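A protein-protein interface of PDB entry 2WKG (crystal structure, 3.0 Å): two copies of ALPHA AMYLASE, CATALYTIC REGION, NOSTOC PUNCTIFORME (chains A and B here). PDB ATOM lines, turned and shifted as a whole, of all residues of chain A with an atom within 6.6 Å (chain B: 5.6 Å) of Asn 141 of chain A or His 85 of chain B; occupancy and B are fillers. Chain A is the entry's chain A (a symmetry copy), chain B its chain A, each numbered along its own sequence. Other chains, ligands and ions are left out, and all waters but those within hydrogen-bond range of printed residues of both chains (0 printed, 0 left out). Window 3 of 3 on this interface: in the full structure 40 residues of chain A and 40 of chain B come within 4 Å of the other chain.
The side-chain carboxylate of Asp 137 of chain A lies within hydrogen-bond range of the backbone NH of Ser 83 of chain B (2.8 Å). ND1 of His 85 of chain B sits close to ND2 of Asn 141 of chain A, 3.4 Å away.
The backbone carbonyl oxygen (O) of His 85 of chain B lies within hydrogen-bond range of the side-chain hydroxyl (OG) of Ser 81 of chain B (3.5 Å). OG of Ser 145 of chain A lies within hydrogen-bond range of OD1 of Asp 137 of chain A (2.6 Å).
Among the printed residues, pairs that only touch across the chains: Pro 146 of chain A with Ser 83 of chain B, Asn 141 of chain A with Ser 83 of chain B, Asn 141 of chain A with Asn 84 of chain B, Asp 137 of chain A with Ala 82 of chain B, Glu 140 of chain A with Ala 82 of chain B and Glu 140 of chain A with His 88 of chain B.
Printed residues of chain B within 4 Å of Glu 140 of chain A: Ala 82 (3.9 Å) and His 88 (3.9 Å). Of chain B, only Ser 83, Asn 84 and His 85 come within 4 Å of Asn 141 of chain A. Printed residues of chain B within 4 Å of Pro 146 of chain A: Ser 83. Of the printed residues of chain A, Ser 83 of chain B touches Asp 137, Asn 141 and Pro 146. His 85 of chain B touches just one residue of chain A: Asn 141 (3.0 Å). Of the printed residues of chain A, His 88 of chain B touches Glu 140 (3.9 Å). The nearest printed residue of chain B that does not touch Asp 137 of chain A is Ser 81 of chain B (4.7 Å).
Hydrophobic or aromatic side chains of chain B that line the printed part of chain A: Ala 82, His 85 and His 88. Along chain B the printed residues that touch a printed residue of chain A span positions 82 to 88. Among the printed residues, no Asp or Glu carboxylate lies within 4 Å of a Lys or Arg side-chain nitrogen of the other chain.
No position is printed for both chains.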
ATOM      1  N   HIS A 136     -27.775  -4.744 -20.717  1.00  0.00           N
ATOM      2  CA  HIS A 136     -27.488  -6.151 -20.976  1.00  0.00           C
ATOM      3  C   HIS A 136     -26.062  -6.277 -21.512  1.00  0.00           C
ATOM      4  O   HIS A 136     -25.263  -7.065 -21.003  1.00  0.00           O
ATOM      5  CB  HIS A 136     -28.487  -6.696 -22.004  1.00  0.00           C
ATOM      6  CG  HIS A 136     -28.105  -8.022 -22.593  1.00  0.00           C
ATOM      7  ND1 HIS A 136     -28.111  -9.193 -21.867  1.00  0.00           N
ATOM      8  CD2 HIS A 136     -27.700  -8.354 -23.840  1.00  0.00           C
ATOM      9  CE1 HIS A 136     -27.725 -10.189 -22.642  1.00  0.00           C
ATOM     10  NE2 HIS A 136     -27.470  -9.708 -23.845  1.00  0.00           N
ATOM     11  N   ASP A 137     -25.750  -5.488 -22.536  1.00  0.00           N
ATOM     12  CA  ASP A 137     -24.423  -5.504 -23.135  1.00  0.00           C
ATOM     13  C   ASP A 137     -23.376  -5.362 -22.040  1.00  0.00           C
ATOM     14  O   ASP A 137     -22.446  -6.166 -21.949  1.00  0.00           O
ATOM     15  CB  ASP A 137     -24.275  -4.356 -24.134  1.00  0.00           C
ATOM     16  CG  ASP A 137     -23.007  -4.463 -24.966  1.00  0.00           C
ATOM     17  OD1 ASP A 137     -21.896  -4.461 -24.392  1.00  0.00           O
ATOM     18  OD2 ASP A 137     -23.123  -4.548 -26.205  1.00  0.00           O
ATOM     19  N   VAL A 138     -23.526  -4.337 -21.207  1.00  0.00           N
ATOM     20  CA  VAL A 138     -22.586  -4.114 -20.122  1.00  0.00           C
ATOM     21  C   VAL A 138     -22.408  -5.395 -19.323  1.00  0.00           C
ATOM     22  O   VAL A 138     -21.288  -5.879 -19.161  1.00  0.00           O
ATOM     23  CB  VAL A 138     -23.067  -2.990 -19.187  1.00  0.00           C
ATOM     24  CG1 VAL A 138     -22.203  -2.941 -17.943  1.00  0.00           C
ATOM     25  CG2 VAL A 138     -23.003  -1.658 -19.910  1.00  0.00           C
ATOM     26  N   LEU A 139     -23.516  -5.951 -18.840  1.00  0.00           N
ATOM     27  CA  LEU A 139     -23.471  -7.181 -18.060  1.00  0.00           C
ATOM     28  C   LEU A 139     -22.745  -8.301 -18.787  1.00  0.00           C
ATOM     29  O   LEU A 139     -22.010  -9.075 -18.175  1.00  0.00           O
ATOM     30  CB  LEU A 139     -24.881  -7.666 -17.728  1.00  0.00           C
ATOM     31  CG  LEU A 139     -25.803  -6.685 -17.011  1.00  0.00           C
ATOM     32  CD1 LEU A 139     -27.011  -7.445 -16.460  1.00  0.00           C
ATOM     33  CD2 LEU A 139     -25.043  -5.989 -15.889  1.00  0.00           C
ATOM     34  N   GLU A 140     -22.955  -8.384 -20.095  1.00  0.00           N
ATOM     35  CA  GLU A 140     -22.336  -9.430 -20.894  1.00  0.00           C
ATOM     36  C   GLU A 140     -20.874  -9.147 -21.236  1.00  0.00           C
ATOM     37  O   GLU A 140     -20.072 -10.072 -21.313  1.00  0.00           O
ATOM     38  CB  GLU A 140     -23.138  -9.639 -22.187  1.00  0.00           C
ATOM     39  CG  GLU A 140     -23.321 -11.102 -22.576  1.00  0.00           C
ATOM     40  CD  GLU A 140     -24.460 -11.769 -21.834  1.00  0.00           C
ATOM     41  OE1 GLU A 140     -24.750 -11.351 -20.692  1.00  0.00           O
ATOM     42  OE2 GLU A 140     -25.056 -12.719 -22.390  1.00  0.00           O
ATOM     43  N   ASN A 141     -20.523  -7.876 -21.428  1.00  0.00           N
ATOM     44  CA  ASN A 141     -19.150  -7.507 -21.785  1.00  0.00           C
ATOM     45  C   ASN A 141     -18.321  -6.789 -20.718  1.00  0.00           C
ATOM     46  O   ASN A 141     -17.247  -6.256 -21.015  1.00  0.00           O
ATOM     47  CB  ASN A 141     -19.153  -6.655 -23.059  1.00  0.00           C
ATOM     48  CG  ASN A 141     -19.432  -7.471 -24.300  1.00  0.00           C
ATOM     49  OD1 ASN A 141     -19.473  -6.944 -25.411  1.00  0.00           O
ATOM     50  ND2 ASN A 141     -19.622  -8.771 -24.117  1.00  0.00           N
ATOM     51  N   GLY A 142     -18.808  -6.775 -19.484  1.00  0.00           N
ATOM     52  CA  GLY A 142     -18.074  -6.112 -18.422  1.00  0.00           C
ATOM     53  C   GLY A 142     -17.354  -4.842 -18.853  1.00  0.00           C
ATOM     54  O   GLY A 142     -17.908  -4.034 -19.594  1.00  0.00           O
ATOM     55  N   PRO A 143     -16.106  -4.641 -18.405  1.00  0.00           N
ATOM     56  CA  PRO A 143     -15.305  -3.460 -18.743  1.00  0.00           C
ATOM     57  C   PRO A 143     -15.229  -3.131 -20.229  1.00  0.00           C
ATOM     58  O   PRO A 143     -15.012  -1.978 -20.596  1.00  0.00           O
ATOM     59  CB  PRO A 143     -13.936  -3.806 -18.174  1.00  0.00           C
ATOM     60  CG  PRO A 143     -14.277  -4.618 -16.973  1.00  0.00           C
ATOM     61  CD  PRO A 143     -15.366  -5.527 -17.490  1.00  0.00           C
ATOM     62  N   HIS A 144     -15.418  -4.137 -21.080  1.00  0.00           N
ATOM     63  CA  HIS A 144     -15.325  -3.940 -22.526  1.00  0.00           C
ATOM     64  C   HIS A 144     -16.591  -3.499 -23.248  1.00  0.00           C
ATOM     65  O   HIS A 144     -16.543  -3.222 -24.446  1.00  0.00           O
ATOM     66  CB  HIS A 144     -14.798  -5.210 -23.192  1.00  0.00           C
ATOM     67  CG  HIS A 144     -13.466  -5.652 -22.673  1.00  0.00           C
ATOM     68  ND1 HIS A 144     -12.357  -4.835 -22.677  1.00  0.00           N
ATOM     69  CD2 HIS A 144     -13.067  -6.825 -22.126  1.00  0.00           C
ATOM     70  CE1 HIS A 144     -11.333  -5.483 -22.153  1.00  0.00           C
ATOM     71  NE2 HIS A 144     -11.737  -6.694 -21.812  1.00  0.00           N
ATOM     72  N   SER A 145     -17.719  -3.437 -22.546  1.00  0.00           N
ATOM     73  CA  SER A 145     -18.956  -3.006 -23.190  1.00  0.00           C
ATOM     74  C   SER A 145     -18.805  -1.588 -23.725  1.00  0.00           C
ATOM     75  O   SER A 145     -18.255  -0.720 -23.057  1.00  0.00           O
ATOM     76  CB  SER A 145     -20.127  -3.053 -22.219  1.00  0.00           C
ATOM     77  OG  SER A 145     -21.263  -2.437 -22.803  1.00  0.00           O
ATOM     78  N   PRO A 146     -19.298  -1.338 -24.943  1.00  0.00           N
ATOM     79  CA  PRO A 146     -19.237  -0.037 -25.613  1.00  0.00           C
ATOM     80  C   PRO A 146     -20.014   1.066 -24.908  1.00  0.00           C
ATOM     81  O   PRO A 146     -19.740   2.253 -25.100  1.00  0.00           O
ATOM     82  CB  PRO A 146     -19.819  -0.329 -26.994  1.00  0.00           C
ATOM     83  CG  PRO A 146     -19.549  -1.782 -27.187  1.00  0.00           C
ATOM     84  CD  PRO A 146     -19.877  -2.352 -25.838  1.00  0.00           C
ATOM     85  N   VAL A 148     -20.506   1.593 -21.356  1.00  0.00           N
ATOM     86  CA  VAL A 148     -20.334   1.495 -19.913  1.00  0.00           C
ATOM     87  C   VAL A 148     -20.588   2.896 -19.368  1.00  0.00           C
ATOM     88  O   VAL A 148     -21.008   3.073 -18.224  1.00  0.00           O
ATOM     89  CB  VAL A 148     -18.907   1.057 -19.549  1.00  0.00           C
ATOM     90  CG1 VAL A 148     -18.739   1.057 -18.048  1.00  0.00           C
ATOM     91  CG2 VAL A 148     -18.630  -0.324 -20.105  1.00  0.00           C
ATOM     92  N   TRP A 156     -15.828  -2.735 -11.005  1.00  0.00           N
ATOM     93  CA  TRP A 156     -16.117  -4.104 -11.411  1.00  0.00           C
ATOM     94  C   TRP A 156     -15.598  -5.094 -10.390  1.00  0.00           C
ATOM     95  O   TRP A 156     -14.679  -4.793  -9.640  1.00  0.00           O
ATOM     96  CB  TRP A 156     -15.499  -4.374 -12.780  1.00  0.00           C
ATOM     97  CG  TRP A 156     -16.188  -3.611 -13.875  1.00  0.00           C
ATOM     98  CD1 TRP A 156     -17.395  -3.908 -14.453  1.00  0.00           C
ATOM     99  CD2 TRP A 156     -15.732  -2.404 -14.497  1.00  0.00           C
ATOM    100  NE1 TRP A 156     -17.714  -2.960 -15.396  1.00  0.00           N
ATOM    101  CE2 TRP A 156     -16.712  -2.026 -15.443  1.00  0.00           C
ATOM    102  CE3 TRP A 156     -14.590  -1.604 -14.345  1.00  0.00           C
ATOM    103  CZ2 TRP A 156     -16.581  -0.881 -16.238  1.00  0.00           C
ATOM    104  CZ3 TRP A 156     -14.461  -0.463 -15.136  1.00  0.00           C
ATOM    105  CH2 TRP A 156     -15.453  -0.115 -16.070  1.00  0.00           C
ATOM    106  N   SER B  81     -27.733  -8.325 -30.516  1.00  0.00           N
ATOM    107  CA  SER B  81     -27.151  -9.125 -29.444  1.00  0.00           C
ATOM    108  C   SER B  81     -26.046  -8.359 -28.724  1.00  0.00           C
ATOM    109  O   SER B  81     -25.718  -7.231 -29.092  1.00  0.00           O
ATOM    110  CB  SER B  81     -26.604 -10.443 -29.995  1.00  0.00           C
ATOM    111  OG  SER B  81     -25.734 -10.216 -31.092  1.00  0.00           O
ATOM    112  N   ALA B  82     -25.475  -8.980 -27.698  1.00  0.00           N
ATOM    113  CA  ALA B  82     -24.318  -8.420 -27.010  1.00  0.00           C
ATOM    114  C   ALA B  82     -23.267  -7.936 -28.005  1.00  0.00           C
ATOM    115  O   ALA B  82     -23.074  -8.538 -29.061  1.00  0.00           O
ATOM    116  CB  ALA B  82     -23.718  -9.442 -26.058  1.00  0.00           C
ATOM    117  N   SER B  83     -22.591  -6.845 -27.661  1.00  0.00           N
ATOM    118  CA  SER B  83     -21.762  -6.123 -28.618  1.00  0.00           C
ATOM    119  C   SER B  83     -20.843  -7.074 -29.378  1.00  0.00           C
ATOM    120  O   SER B  83     -20.468  -6.809 -30.520  1.00  0.00           O
ATOM    121  CB  SER B  83     -20.935  -5.048 -27.909  1.00  0.00           C
ATOM    122  OG  SER B  83     -19.938  -4.523 -28.767  1.00  0.00           O
ATOM    123  N   ASN B  84     -20.483  -8.181 -28.737  1.00  0.00           N
ATOM    124  CA  ASN B  84     -19.529  -9.122 -29.309  1.00  0.00           C
ATOM    125  C   ASN B  84     -19.940 -10.573 -29.076  1.00  0.00           C
ATOM    126  O   ASN B  84     -19.092 -11.455 -28.942  1.00  0.00           O
ATOM    127  CB  ASN B  84     -18.128  -8.877 -28.744  1.00  0.00           C
ATOM    128  CG  ASN B  84     -17.036  -9.451 -29.624  1.00  0.00           C
ATOM    129  OD1 ASN B  84     -15.848  -9.296 -29.339  1.00  0.00           O
ATOM    130  ND2 ASN B  84     -17.433 -10.120 -30.699  1.00  0.00           N
ATOM    131  N   HIS B  85     -21.247 -10.812 -29.031  1.00  0.00           N
ATOM    132  CA  HIS B  85     -21.773 -12.167 -28.911  1.00  0.00           C
ATOM    133  C   HIS B  85     -22.928 -12.397 -29.881  1.00  0.00           C
ATOM    134  O   HIS B  85     -24.018 -12.803 -29.478  1.00  0.00           O
ATOM    135  CB  HIS B  85     -22.230 -12.438 -27.476  1.00  0.00           C
ATOM    136  CG  HIS B  85     -21.125 -12.373 -26.468  1.00  0.00           C
ATOM    137  ND1 HIS B  85     -20.272 -11.295 -26.368  1.00  0.00           N
ATOM    138  CD2 HIS B  85     -20.734 -13.252 -25.516  1.00  0.00           C
ATOM    139  CE1 HIS B  85     -19.403 -11.514 -25.397  1.00  0.00           C
ATOM    140  NE2 HIS B  85     -19.662 -12.694 -24.864  1.00  0.00           N
ATOM    141  N   ARG B  86     -22.681 -12.135 -31.160  1.00  0.00           N
ATOM    142  CA  ARG B  86     -23.741 -12.132 -32.160  1.00  0.00           C
ATOM    143  C   ARG B  86     -24.668 -13.330 -31.984  1.00  0.00           C
ATOM    144  O   ARG B  86     -25.830 -13.292 -32.389  1.00  0.00           O
ATOM    145  CB  ARG B  86     -23.147 -12.129 -33.571  1.00  0.00           C
ATOM    146  CG  ARG B  86     -22.272 -10.924 -33.873  1.00  0.00           C
ATOM    147  CD  ARG B  86     -23.093  -9.770 -34.426  1.00  0.00           C
ATOM    148  NE  ARG B  86     -23.590  -8.896 -33.367  1.00  0.00           N
ATOM    149  CZ  ARG B  86     -23.542  -7.568 -33.411  1.00  0.00           C
ATOM    150  NH1 ARG B  86     -23.020  -6.956 -34.465  1.00  0.00           N
ATOM    151  NH2 ARG B  86     -24.018  -6.852 -32.402  1.00  0.00           N
ATOM    152  N   TYR B  87     -24.146 -14.392 -31.378  1.00  0.00           N
ATOM    153  CA  TYR B  87     -24.851 -15.667 -31.327  1.00  0.00           C
ATOM    154  C   TYR B  87     -25.704 -15.775 -30.068  1.00  0.00           C
ATOM    155  O   TYR B  87     -26.453 -16.737 -29.895  1.00  0.00           O
ATOM    156  CB  TYR B  87     -23.858 -16.830 -31.390  1.00  0.00           C
ATOM    157  CG  TYR B  87     -23.464 -17.223 -32.796  1.00  0.00           C
ATOM    158  CD1 TYR B  87     -24.184 -18.179 -33.499  1.00  0.00           C
ATOM    159  CD2 TYR B  87     -22.370 -16.636 -33.419  1.00  0.00           C
ATOM    160  CE1 TYR B  87     -23.827 -18.541 -34.784  1.00  0.00           C
ATOM    161  CE2 TYR B  87     -22.005 -16.992 -34.706  1.00  0.00           C
ATOM    162  CZ  TYR B  87     -22.737 -17.944 -35.382  1.00  0.00           C
ATOM    163  OH  TYR B  87     -22.377 -18.301 -36.661  1.00  0.00           O
ATOM    164  N   HIS B  88     -25.587 -14.782 -29.192  1.00  0.00           N
ATOM    165  CA  HIS B  88     -26.417 -14.715 -27.994  1.00  0.00           C
ATOM    166  C   HIS B  88     -27.528 -13.712 -28.309  1.00  0.00           C
ATOM    167  O   HIS B  88     -27.512 -12.579 -27.828  1.00  0.00           O
ATOM    168  CB  HIS B  88     -25.615 -14.222 -26.783  1.00  0.00           C
ATOM    169  CG  HIS B  88     -24.357 -14.994 -26.513  1.00  0.00           C
ATOM    170  ND1 HIS B  88     -23.823 -15.119 -25.248  1.00  0.00           N
ATOM    171  CD2 HIS B  88     -23.499 -15.634 -27.344  1.00  0.00           C
ATOM    172  CE1 HIS B  88     -22.694 -15.800 -25.310  1.00  0.00           C
ATOM    173  NE2 HIS B  88     -22.474 -16.123 -26.571  1.00  0.00           N
ATOM    174  N   THR B  89     -28.491 -14.139 -29.121  1.00  0.00           N
ATOM    175  CA  THR B  89     -29.588 -13.278 -29.539  1.00  0.00           C
ATOM    176  C   THR B  89     -30.301 -12.565 -28.404  1.00  0.00           C
ATOM    177  O   THR B  89     -30.606 -13.158 -27.375  1.00  0.00           O
ATOM    178  CB  THR B  89     -30.642 -14.059 -30.343  1.00  0.00           C
ATOM    179  OG1 THR B  89     -29.992 -14.873 -31.323  1.00  0.00           O
ATOM    180  CG2 THR B  89     -31.579 -13.094 -31.058  1.00  0.00           C
